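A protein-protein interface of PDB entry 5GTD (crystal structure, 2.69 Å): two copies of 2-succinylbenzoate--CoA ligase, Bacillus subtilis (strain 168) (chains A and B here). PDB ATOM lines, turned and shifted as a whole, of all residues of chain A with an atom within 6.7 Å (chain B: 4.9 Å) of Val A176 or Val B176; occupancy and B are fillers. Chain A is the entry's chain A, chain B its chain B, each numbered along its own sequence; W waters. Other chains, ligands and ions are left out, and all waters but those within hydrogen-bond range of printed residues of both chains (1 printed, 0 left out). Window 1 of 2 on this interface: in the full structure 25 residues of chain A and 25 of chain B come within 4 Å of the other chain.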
ATOM      1  N   HIS A 171     -19.848  15.302 -20.057  1.00  0.00           N
ATOM      2  CA  HIS A 171     -20.474  16.614 -19.950  1.00  0.00           C
ATOM      3  C   HIS A 171     -21.356  16.716 -18.711  1.00  0.00           C
ATOM      4  O   HIS A 171     -21.358  17.741 -18.025  1.00  0.00           O
ATOM      5  CB  HIS A 171     -21.296  16.925 -21.201  1.00  0.00           C
ATOM      6  CG  HIS A 171     -20.470  17.088 -22.440  1.00  0.00           C
ATOM      7  ND1 HIS A 171     -19.399  17.948 -22.510  1.00  0.00           N
ATOM      8  CD2 HIS A 171     -20.565  16.501 -23.656  1.00  0.00           C
ATOM      9  CE1 HIS A 171     -18.864  17.885 -23.718  1.00  0.00           C
ATOM     10  NE2 HIS A 171     -19.553  17.016 -24.432  1.00  0.00           N
ATOM     11  N   TYR A 172     -22.103  15.653 -18.428  1.00  0.00           N
ATOM     12  CA  TYR A 172     -22.964  15.629 -17.252  1.00  0.00           C
ATOM     13  C   TYR A 172     -22.157  15.809 -15.971  1.00  0.00           C
ATOM     14  O   TYR A 172     -22.526  16.603 -15.109  1.00  0.00           O
ATOM     15  CB  TYR A 172     -23.763  14.322 -17.183  1.00  0.00           C
ATOM     16  CG  TYR A 172     -24.470  14.122 -15.857  1.00  0.00           C
ATOM     17  CD1 TYR A 172     -25.694  14.726 -15.605  1.00  0.00           C
ATOM     18  CD2 TYR A 172     -23.906  13.337 -14.853  1.00  0.00           C
ATOM     19  CE1 TYR A 172     -26.340  14.554 -14.394  1.00  0.00           C
ATOM     20  CE2 TYR A 172     -24.545  13.160 -13.637  1.00  0.00           C
ATOM     21  CZ  TYR A 172     -25.762  13.769 -13.414  1.00  0.00           C
ATOM     22  OH  TYR A 172     -26.406  13.595 -12.209  1.00  0.00           O
ATOM     23  N   PHE A 173     -21.057  15.073 -15.846  1.00  0.00           N
ATOM     24  CA  PHE A 173     -20.275  15.104 -14.614  1.00  0.00           C
ATOM     25  C   PHE A 173     -19.453  16.377 -14.484  1.00  0.00           C
ATOM     26  O   PHE A 173     -19.136  16.810 -13.373  1.00  0.00           O
ATOM     27  CB  PHE A 173     -19.374  13.869 -14.517  1.00  0.00           C
ATOM     28  CG  PHE A 173     -20.093  12.648 -14.029  1.00  0.00           C
ATOM     29  CD1 PHE A 173     -20.505  12.560 -12.710  1.00  0.00           C
ATOM     30  CD2 PHE A 173     -20.375  11.596 -14.886  1.00  0.00           C
ATOM     31  CE1 PHE A 173     -21.178  11.445 -12.253  1.00  0.00           C
ATOM     32  CE2 PHE A 173     -21.046  10.478 -14.436  1.00  0.00           C
ATOM     33  CZ  PHE A 173     -21.448  10.401 -13.118  1.00  0.00           C
ATOM     34  N   SER A 174     -19.114  16.978 -15.620  1.00  0.00           N
ATOM     35  CA  SER A 174     -18.491  18.293 -15.619  1.00  0.00           C
ATOM     36  C   SER A 174     -19.445  19.306 -14.993  1.00  0.00           C
ATOM     37  O   SER A 174     -19.078  20.038 -14.072  1.00  0.00           O
ATOM     38  CB  SER A 174     -18.117  18.719 -17.037  1.00  0.00           C
ATOM     39  OG  SER A 174     -17.392  19.935 -17.029  1.00  0.00           O
ATOM     40  N   ALA A 175     -20.679  19.322 -15.492  1.00  0.00           N
ATOM     41  CA  ALA A 175     -21.691  20.264 -15.028  1.00  0.00           C
ATOM     42  C   ALA A 175     -21.979  20.082 -13.541  1.00  0.00           C
ATOM     43  O   ALA A 175     -22.099  21.055 -12.798  1.00  0.00           O
ATOM     44  CB  ALA A 175     -22.973  20.108 -15.843  1.00  0.00           C
ATOM     45  N   VAL A 176     -22.075  18.828 -13.112  1.00  0.00           N
ATOM     46  CA  VAL A 176     -22.390  18.517 -11.725  1.00  0.00           C
ATOM     47  C   VAL A 176     -21.258  18.917 -10.774  1.00  0.00           C
ATOM     48  O   VAL A 176     -21.495  19.603  -9.773  1.00  0.00           O
ATOM     49  CB  VAL A 176     -22.706  17.020 -11.556  1.00  0.00           C
ATOM     50  CG1 VAL A 176     -22.821  16.659 -10.082  1.00  0.00           C
ATOM     51  CG2 VAL A 176     -23.988  16.669 -12.295  1.00  0.00           C
ATOM     52  N   SER A 177     -20.034  18.501 -11.092  1.00  0.00           N
ATOM     53  CA  SER A 177     -18.877  18.808 -10.250  1.00  0.00           C
ATOM     54  C   SER A 177     -18.679  20.312 -10.075  1.00  0.00           C
ATOM     55  O   SER A 177     -18.354  20.781  -8.982  1.00  0.00           O
ATOM     56  CB  SER A 177     -17.604  18.193 -10.834  1.00  0.00           C
ATOM     57  OG  SER A 177     -17.621  16.784 -10.718  1.00  0.00           O
ATOM     58  N   SER A 178     -18.873  21.053 -11.158  1.00  0.00           N
ATOM     59  CA  SER A 178     -18.739  22.500 -11.134  1.00  0.00           C
ATOM     60  C   SER A 178     -19.790  23.101 -10.205  1.00  0.00           C
ATOM     61  O   SER A 178     -19.507  24.024  -9.435  1.00  0.00           O
ATOM     62  CB  SER A 178     -18.873  23.073 -12.551  1.00  0.00           C
ATOM     63  OG  SER A 178     -18.533  24.447 -12.593  1.00  0.00           O
ATOM     64  N   ALA A 179     -20.999  22.554 -10.266  1.00  0.00           N
ATOM     65  CA  ALA A 179     -22.100  23.043  -9.447  1.00  0.00           C
ATOM     66  C   ALA A 179     -21.883  22.722  -7.969  1.00  0.00           C
ATOM     67  O   ALA A 179     -22.252  23.508  -7.099  1.00  0.00           O
ATOM     68  CB  ALA A 179     -23.407  22.460  -9.928  1.00  0.00           C
ATOM     69  N   LEU A 180     -21.281  21.568  -7.689  1.00  0.00           N
ATOM     70  CA  LEU A 180     -20.945  21.199  -6.316  1.00  0.00           C
ATOM     71  C   LEU A 180     -19.854  22.109  -5.769  1.00  0.00           C
ATOM     72  O   LEU A 180     -19.676  22.231  -4.558  1.00  0.00           O
ATOM     73  CB  LEU A 180     -20.492  19.739  -6.234  1.00  0.00           C
ATOM     74  CG  LEU A 180     -21.559  18.668  -6.444  1.00  0.00           C
ATOM     75  CD1 LEU A 180     -20.921  17.293  -6.465  1.00  0.00           C
ATOM     76  CD2 LEU A 180     -22.628  18.755  -5.369  1.00  0.00           C
ATOM     77  N   ASN A 181     -19.118  22.742  -6.672  1.00  0.00           N
ATOM     78  CA  ASN A 181     -18.030  23.623  -6.285  1.00  0.00           C
ATOM     79  C   ASN A 181     -18.480  25.081  -6.191  1.00  0.00           C
ATOM     80  O   ASN A 181     -18.099  25.793  -5.262  1.00  0.00           O
ATOM     81  CB  ASN A 181     -16.872  23.483  -7.273  1.00  0.00           C
ATOM     82  CG  ASN A 181     -15.690  24.354  -6.914  1.00  0.00           C
ATOM     83  OD1 ASN A 181     -15.257  25.190  -7.708  1.00  0.00           O
ATOM     84  ND2 ASN A 181     -15.163  24.172  -5.707  1.00  0.00           N
ATOM     85  N   ILE A 184     -25.473  26.357  -6.762  1.00  0.00           N
ATOM     86  CA  ILE A 184     -26.476  26.820  -7.719  1.00  0.00           C
ATOM     87  C   ILE A 184     -27.614  27.554  -7.028  1.00  0.00           C
ATOM     88  O   ILE A 184     -28.207  27.042  -6.078  1.00  0.00           O
ATOM     89  CB  ILE A 184     -27.108  25.670  -8.526  1.00  0.00           C
ATOM     90  CG1 ILE A 184     -26.128  24.521  -8.741  1.00  0.00           C
ATOM     91  CG2 ILE A 184     -27.646  26.188  -9.854  1.00  0.00           C
ATOM     92  CD1 ILE A 184     -26.794  23.298  -9.326  1.00  0.00           C
ATOM     93  N   LYS A 207     -24.491  22.844 -18.895  1.00  0.00           N
ATOM     94  CA  LYS A 207     -24.829  23.418 -17.595  1.00  0.00           C
ATOM     95  C   LYS A 207     -26.249  23.973 -17.642  1.00  0.00           C
ATOM     96  O   LYS A 207     -27.020  23.808 -16.702  1.00  0.00           O
ATOM     97  CB  LYS A 207     -23.856  24.536 -17.199  1.00  0.00           C
ATOM     98  CG  LYS A 207     -22.450  24.098 -16.816  1.00  0.00           C
ATOM     99  CD  LYS A 207     -21.663  25.287 -16.266  1.00  0.00           C
ATOM    100  CE  LYS A 207     -20.202  24.954 -15.996  1.00  0.00           C
ATOM    101  NZ  LYS A 207     -19.389  24.854 -17.243  1.00  0.00           N
ATOM    102  N   ILE A 210     -29.121  21.185 -17.773  1.00  0.00           N
ATOM    103  CA  ILE A 210     -29.055  20.345 -16.583  1.00  0.00           C
ATOM    104  C   ILE A 210     -29.451  21.137 -15.332  1.00  0.00           C
ATOM    105  O   ILE A 210     -30.218  20.643 -14.499  1.00  0.00           O
ATOM    106  CB  ILE A 210     -27.651  19.736 -16.401  1.00  0.00           C
ATOM    107  CG1 ILE A 210     -27.384  18.693 -17.487  1.00  0.00           C
ATOM    108  CG2 ILE A 210     -27.515  19.088 -15.036  1.00  0.00           C
ATOM    109  CD1 ILE A 210     -25.990  18.106 -17.441  1.00  0.00           C
ATOM    110  N   TYR A 211     -28.941  22.363 -15.207  1.00  0.00           N
ATOM    111  CA  TYR A 211     -29.294  23.217 -14.071  1.00  0.00           C
ATOM    112  C   TYR A 211     -30.686  23.815 -14.231  1.00  0.00           C
ATOM    113  O   TYR A 211     -31.352  24.139 -13.247  1.00  0.00           O
ATOM    114  CB  TYR A 211     -28.308  24.376 -13.894  1.00  0.00           C
ATOM    115  CG  TYR A 211     -26.854  24.020 -13.694  1.00  0.00           C
ATOM    116  CD1 TYR A 211     -26.446  22.713 -13.463  1.00  0.00           C
ATOM    117  CD2 TYR A 211     -25.883  25.012 -13.731  1.00  0.00           C
ATOM    118  CE1 TYR A 211     -25.108  22.408 -13.286  1.00  0.00           C
ATOM    119  CE2 TYR A 211     -24.553  24.720 -13.552  1.00  0.00           C
ATOM    120  CZ  TYR A 211     -24.167  23.419 -13.331  1.00  0.00           C
ATOM    121  OH  TYR A 211     -22.833  23.140 -13.154  1.00  0.00           O
ATOM    122  N   PHE A 317     -14.939  17.962  -7.119  1.00  0.00           N
ATOM    123  CA  PHE A 317     -15.423  16.729  -6.512  1.00  0.00           C
ATOM    124  C   PHE A 317     -15.525  15.632  -7.564  1.00  0.00           C
ATOM    125  O   PHE A 317     -15.823  15.915  -8.726  1.00  0.00           O
ATOM    126  CB  PHE A 317     -16.774  16.948  -5.831  1.00  0.00           C
ATOM    127  CG  PHE A 317     -17.018  16.033  -4.666  1.00  0.00           C
ATOM    128  CD1 PHE A 317     -16.520  16.343  -3.410  1.00  0.00           C
ATOM    129  CD2 PHE A 317     -17.745  14.865  -4.823  1.00  0.00           C
ATOM    130  CE1 PHE A 317     -16.742  15.504  -2.331  1.00  0.00           C
ATOM    131  CE2 PHE A 317     -17.972  14.021  -3.747  1.00  0.00           C
ATOM    132  CZ  PHE A 317     -17.468  14.342  -2.501  1.00  0.00           C
ATOM    133  N   SER A 318     -15.242  14.399  -7.139  1.00  0.00           N
ATOM    134  CA  SER A 318     -15.196  13.201  -7.990  1.00  0.00           C
ATOM    135  C   SER A 318     -13.925  13.136  -8.840  1.00  0.00           C
ATOM    136  O   SER A 318     -13.648  12.114  -9.465  1.00  0.00           O
ATOM    137  CB  SER A 318     -16.428  13.110  -8.904  1.00  0.00           C
ATOM    138  OG  SER A 318     -17.618  13.427  -8.205  1.00  0.00           O
ATOM    139  N   TYR B 172     -25.226   8.933  -4.438  1.00  0.00           N
ATOM    140  CA  TYR B 172     -24.625  10.079  -5.111  1.00  0.00           C
ATOM    141  C   TYR B 172     -25.636  10.771  -6.020  1.00  0.00           C
ATOM    142  O   TYR B 172     -25.789  11.992  -5.969  1.00  0.00           O
ATOM    143  CB  TYR B 172     -23.396   9.659  -5.924  1.00  0.00           C
ATOM    144  CG  TYR B 172     -22.911  10.724  -6.893  1.00  0.00           C
ATOM    145  CD1 TYR B 172     -22.036  11.723  -6.484  1.00  0.00           C
ATOM    146  CD2 TYR B 172     -23.333  10.726  -8.219  1.00  0.00           C
ATOM    147  CE1 TYR B 172     -21.595  12.697  -7.371  1.00  0.00           C
ATOM    148  CE2 TYR B 172     -22.903  11.693  -9.106  1.00  0.00           C
ATOM    149  CZ  TYR B 172     -22.035  12.673  -8.680  1.00  0.00           C
ATOM    150  OH  TYR B 172     -21.616  13.626  -9.578  1.00  0.00           O
ATOM    151  N   PHE B 173     -26.320   9.993  -6.853  1.00  0.00           N
ATOM    152  CA  PHE B 173     -27.264  10.577  -7.798  1.00  0.00           C
ATOM    153  C   PHE B 173     -28.479  11.125  -7.069  1.00  0.00           C
ATOM    154  O   PHE B 173     -29.106  12.082  -7.524  1.00  0.00           O
ATOM    155  CB  PHE B 173     -27.674   9.556  -8.863  1.00  0.00           C
ATOM    156  CG  PHE B 173     -26.637   9.360  -9.929  1.00  0.00           C
ATOM    157  CD1 PHE B 173     -26.391  10.358 -10.860  1.00  0.00           C
ATOM    158  CD2 PHE B 173     -25.893   8.193  -9.991  1.00  0.00           C
ATOM    159  CE1 PHE B 173     -25.430  10.194 -11.840  1.00  0.00           C
ATOM    160  CE2 PHE B 173     -24.928   8.021 -10.965  1.00  0.00           C
ATOM    161  CZ  PHE B 173     -24.695   9.025 -11.893  1.00  0.00           C
ATOM    162  N   SER B 174     -28.797  10.528  -5.928  1.00  0.00           N
ATOM    163  CA  SER B 174     -29.833  11.065  -5.059  1.00  0.00           C
ATOM    164  C   SER B 174     -29.462  12.480  -4.621  1.00  0.00           C
ATOM    165  O   SER B 174     -30.251  13.415  -4.773  1.00  0.00           O
ATOM    166  CB  SER B 174     -30.035  10.165  -3.841  1.00  0.00           C
ATOM    167  OG  SER B 174     -30.947  10.743  -2.925  1.00  0.00           O
ATOM    168  N   ALA B 175     -28.251  12.629  -4.091  1.00  0.00           N
ATOM    169  CA  ALA B 175     -27.771  13.914  -3.595  1.00  0.00           C
ATOM    170  C   ALA B 175     -27.685  14.957  -4.709  1.00  0.00           C
ATOM    171  O   ALA B 175     -28.050  16.115  -4.516  1.00  0.00           O
ATOM    172  CB  ALA B 175     -26.415  13.742  -2.920  1.00  0.00           C
ATOM    173  N   VAL B 176     -27.211  14.534  -5.877  1.00  0.00           N
ATOM    174  CA  VAL B 176     -27.049  15.432  -7.014  1.00  0.00           C
ATOM    175  C   VAL B 176     -28.394  15.889  -7.583  1.00  0.00           C
ATOM    176  O   VAL B 176     -28.597  17.078  -7.837  1.00  0.00           O
ATOM    177  CB  VAL B 176     -26.217  14.763  -8.127  1.00  0.00           C
ATOM    178  CG1 VAL B 176     -26.310  15.550  -9.424  1.00  0.00           C
ATOM    179  CG2 VAL B 176     -24.768  14.621  -7.682  1.00  0.00           C
ATOM    180  N   SER B 177     -29.312  14.945  -7.768  1.00  0.00           N
ATOM    181  CA  SER B 177     -30.637  15.255  -8.300  1.00  0.00           C
ATOM    182  C   SER B 177     -31.392  16.263  -7.433  1.00  0.00           C
ATOM    183  O   SER B 177     -32.050  17.164  -7.953  1.00  0.00           O
ATOM    184  CB  SER B 177     -31.467  13.976  -8.445  1.00  0.00           C
ATOM    185  OG  SER B 177     -30.988  13.173  -9.511  1.00  0.00           O
ATOM    186  N   SER B 178     -31.298  16.109  -6.115  1.00  0.00           N
ATOM    187  CA  SER B 178     -31.964  17.022  -5.193  1.00  0.00           C
ATOM    188  C   SER B 178     -31.303  18.397  -5.234  1.00  0.00           C
ATOM    189  O   SER B 178     -31.970  19.423  -5.101  1.00  0.00           O
ATOM    190  CB  SER B 178     -31.946  16.465  -3.768  1.00  0.00           C
ATOM    191  OG  SER B 178     -32.617  17.336  -2.873  1.00  0.00           O
ATOM    192  N   ALA B 179     -29.987  18.409  -5.424  1.00  0.00           N
ATOM    193  CA  ALA B 179     -29.244  19.657  -5.552  1.00  0.00           C
ATOM    194  C   ALA B 179     -29.691  20.422  -6.795  1.00  0.00           C
ATOM    195  O   ALA B 179     -29.937  21.625  -6.738  1.00  0.00           O
ATOM    196  CB  ALA B 179     -27.751  19.384  -5.604  1.00  0.00           C
ATOM    197  N   LEU B 180     -29.804  19.711  -7.913  1.00  0.00           N
ATOM    198  CA  LEU B 180     -30.287  20.300  -9.158  1.00  0.00           C
ATOM    199  C   LEU B 180     -31.712  20.821  -8.995  1.00  0.00           C
ATOM    200  O   LEU B 180     -32.135  21.742  -9.694  1.00  0.00           O
ATOM    201  CB  LEU B 180     -30.227  19.277 -10.294  1.00  0.00           C
ATOM    202  CG  LEU B 180     -28.837  18.762 -10.677  1.00  0.00           C
ATOM    203  CD1 LEU B 180     -28.935  17.690 -11.746  1.00  0.00           C
ATOM    204  CD2 LEU B 180     -27.944  19.903 -11.146  1.00  0.00           C
ATOM    205  N   TYR B 211     -22.017  17.740  -0.906  1.00  0.00           N
ATOM    206  CA  TYR B 211     -22.190  19.187  -1.029  1.00  0.00           C
ATOM    207  C   TYR B 211     -21.085  19.938  -0.288  1.00  0.00           C
ATOM    208  O   TYR B 211     -20.695  21.037  -0.680  1.00  0.00           O
ATOM    209  CB  TYR B 211     -23.540  19.652  -0.466  1.00  0.00           C
ATOM    210  CG  TYR B 211     -24.796  19.052  -1.066  1.00  0.00           C
ATOM    211  CD1 TYR B 211     -24.750  18.185  -2.151  1.00  0.00           C
ATOM    212  CD2 TYR B 211     -26.041  19.361  -0.529  1.00  0.00           C
ATOM    213  CE1 TYR B 211     -25.913  17.646  -2.679  1.00  0.00           C
ATOM    214  CE2 TYR B 211     -27.202  18.829  -1.049  1.00  0.00           C
ATOM    215  CZ  TYR B 211     -27.136  17.975  -2.123  1.00  0.00           C
ATOM    216  OH  TYR B 211     -28.303  17.454  -2.630  1.00  0.00           O
HETATM  217  O   HOH W   1     -19.282  15.034  -9.088  1.00  0.00           O
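Of the 17 printed residues of chain A, 6 touch a printed residue of chain B.
Printed residues of chain A that touch a printed residue of chain B: Tyr A172, Phe A173, Val A176, Leu A180, Ile A210 and Tyr A211.
Hydrophobic or aromatic side chains of chain A within 4 Å of the printed part of chain B: Tyr A172, Phe A173, Val A176, Leu A180, Ile A210 and Tyr A211.
Along chain A the printed residues that touch a printed residue of chain B span positions 172 to 211.
Among the printed residues, 9 pairs touch across the chains.
Of chain B, only Tyr B172 and Val B176 come within 4 Å of Val A176.
Val B176 touches just these residues of chain A: Tyr A172 and Val A176.
Of the printed residues of chain B, Tyr A172 touches Phe B173 and Val B176.
Printed residues of chain B within 4 Å of Tyr A211: Leu B180.
Printed residues of chain A within 4 Å of Leu B180: Ile A210 (3.8 Å) and Tyr A211 (3.9 Å).
Printed residues of chain A within 4 Å of Tyr B211: Leu A180 (3.9 Å).
Ala B179 touches none of the printed residues of chain A.
The nearest residue of chain A that does not touch Val B176 is Leu A180 (4.8 Å).
OG of Ser B177 lies within hydrogen-bond range of O of Phe B173 (2.9 Å).
The side-chain hydroxyl (OH) of Tyr A211 sits close to the backbone NH (N) of Ala A179, 3.5 Å away.
The backbone carbonyl oxygen (O) of Phe A173 lies within hydrogen-bond range of the side-chain hydroxyl (OG) of Ser A177 (3.1 Å).
The backbone NH (N) of Ala B179 is in hydrogen-bond range of the side-chain hydroxyl (OH) of Tyr B211.
Phe B173 touches Tyr A172.
Tyr A172 touches Val B176.
Phe A173 touches Tyr B172 (CE1 to OH, 3.5 Å).
Phe A173 touches Phe B173.
CG1 of Val A176 touches OH of Tyr B172, at 3.3 Å.
Val B176 touches Val A176 (CG2 to CG1, 3.7 Å).
Tyr B211 touches Leu A180.
Leu B180 touches Ile A210 (CD1 to CG2, 3.8 Å).
CD1 of Tyr A211 touches CD2 of Leu B180 (3.9 Å).
Water W1 lies within hydrogen-bond range of OG of Ser A318, OH of Tyr B172 and OG of Ser A177.
Tyr A172 touches Phe B173, and with the chains exchanged Phe A173 touches Tyr B172.
Tyr A172 touches Val B176, and with the chains exchanged Val A176 touches Tyr B172.
Val B176 touches its own counterpart, Val A176.
Leu A180 touches Tyr B211, and with the chains exchanged Tyr A211 touches Leu B180.
Positions printed for both chains: 172, 173, 174, 175, 176, 177, 178, 179, 180 and 211.
Of the 9 pairs that touch across the chains among the printed residues, 8 have their exchanged pair printed and touching as well.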
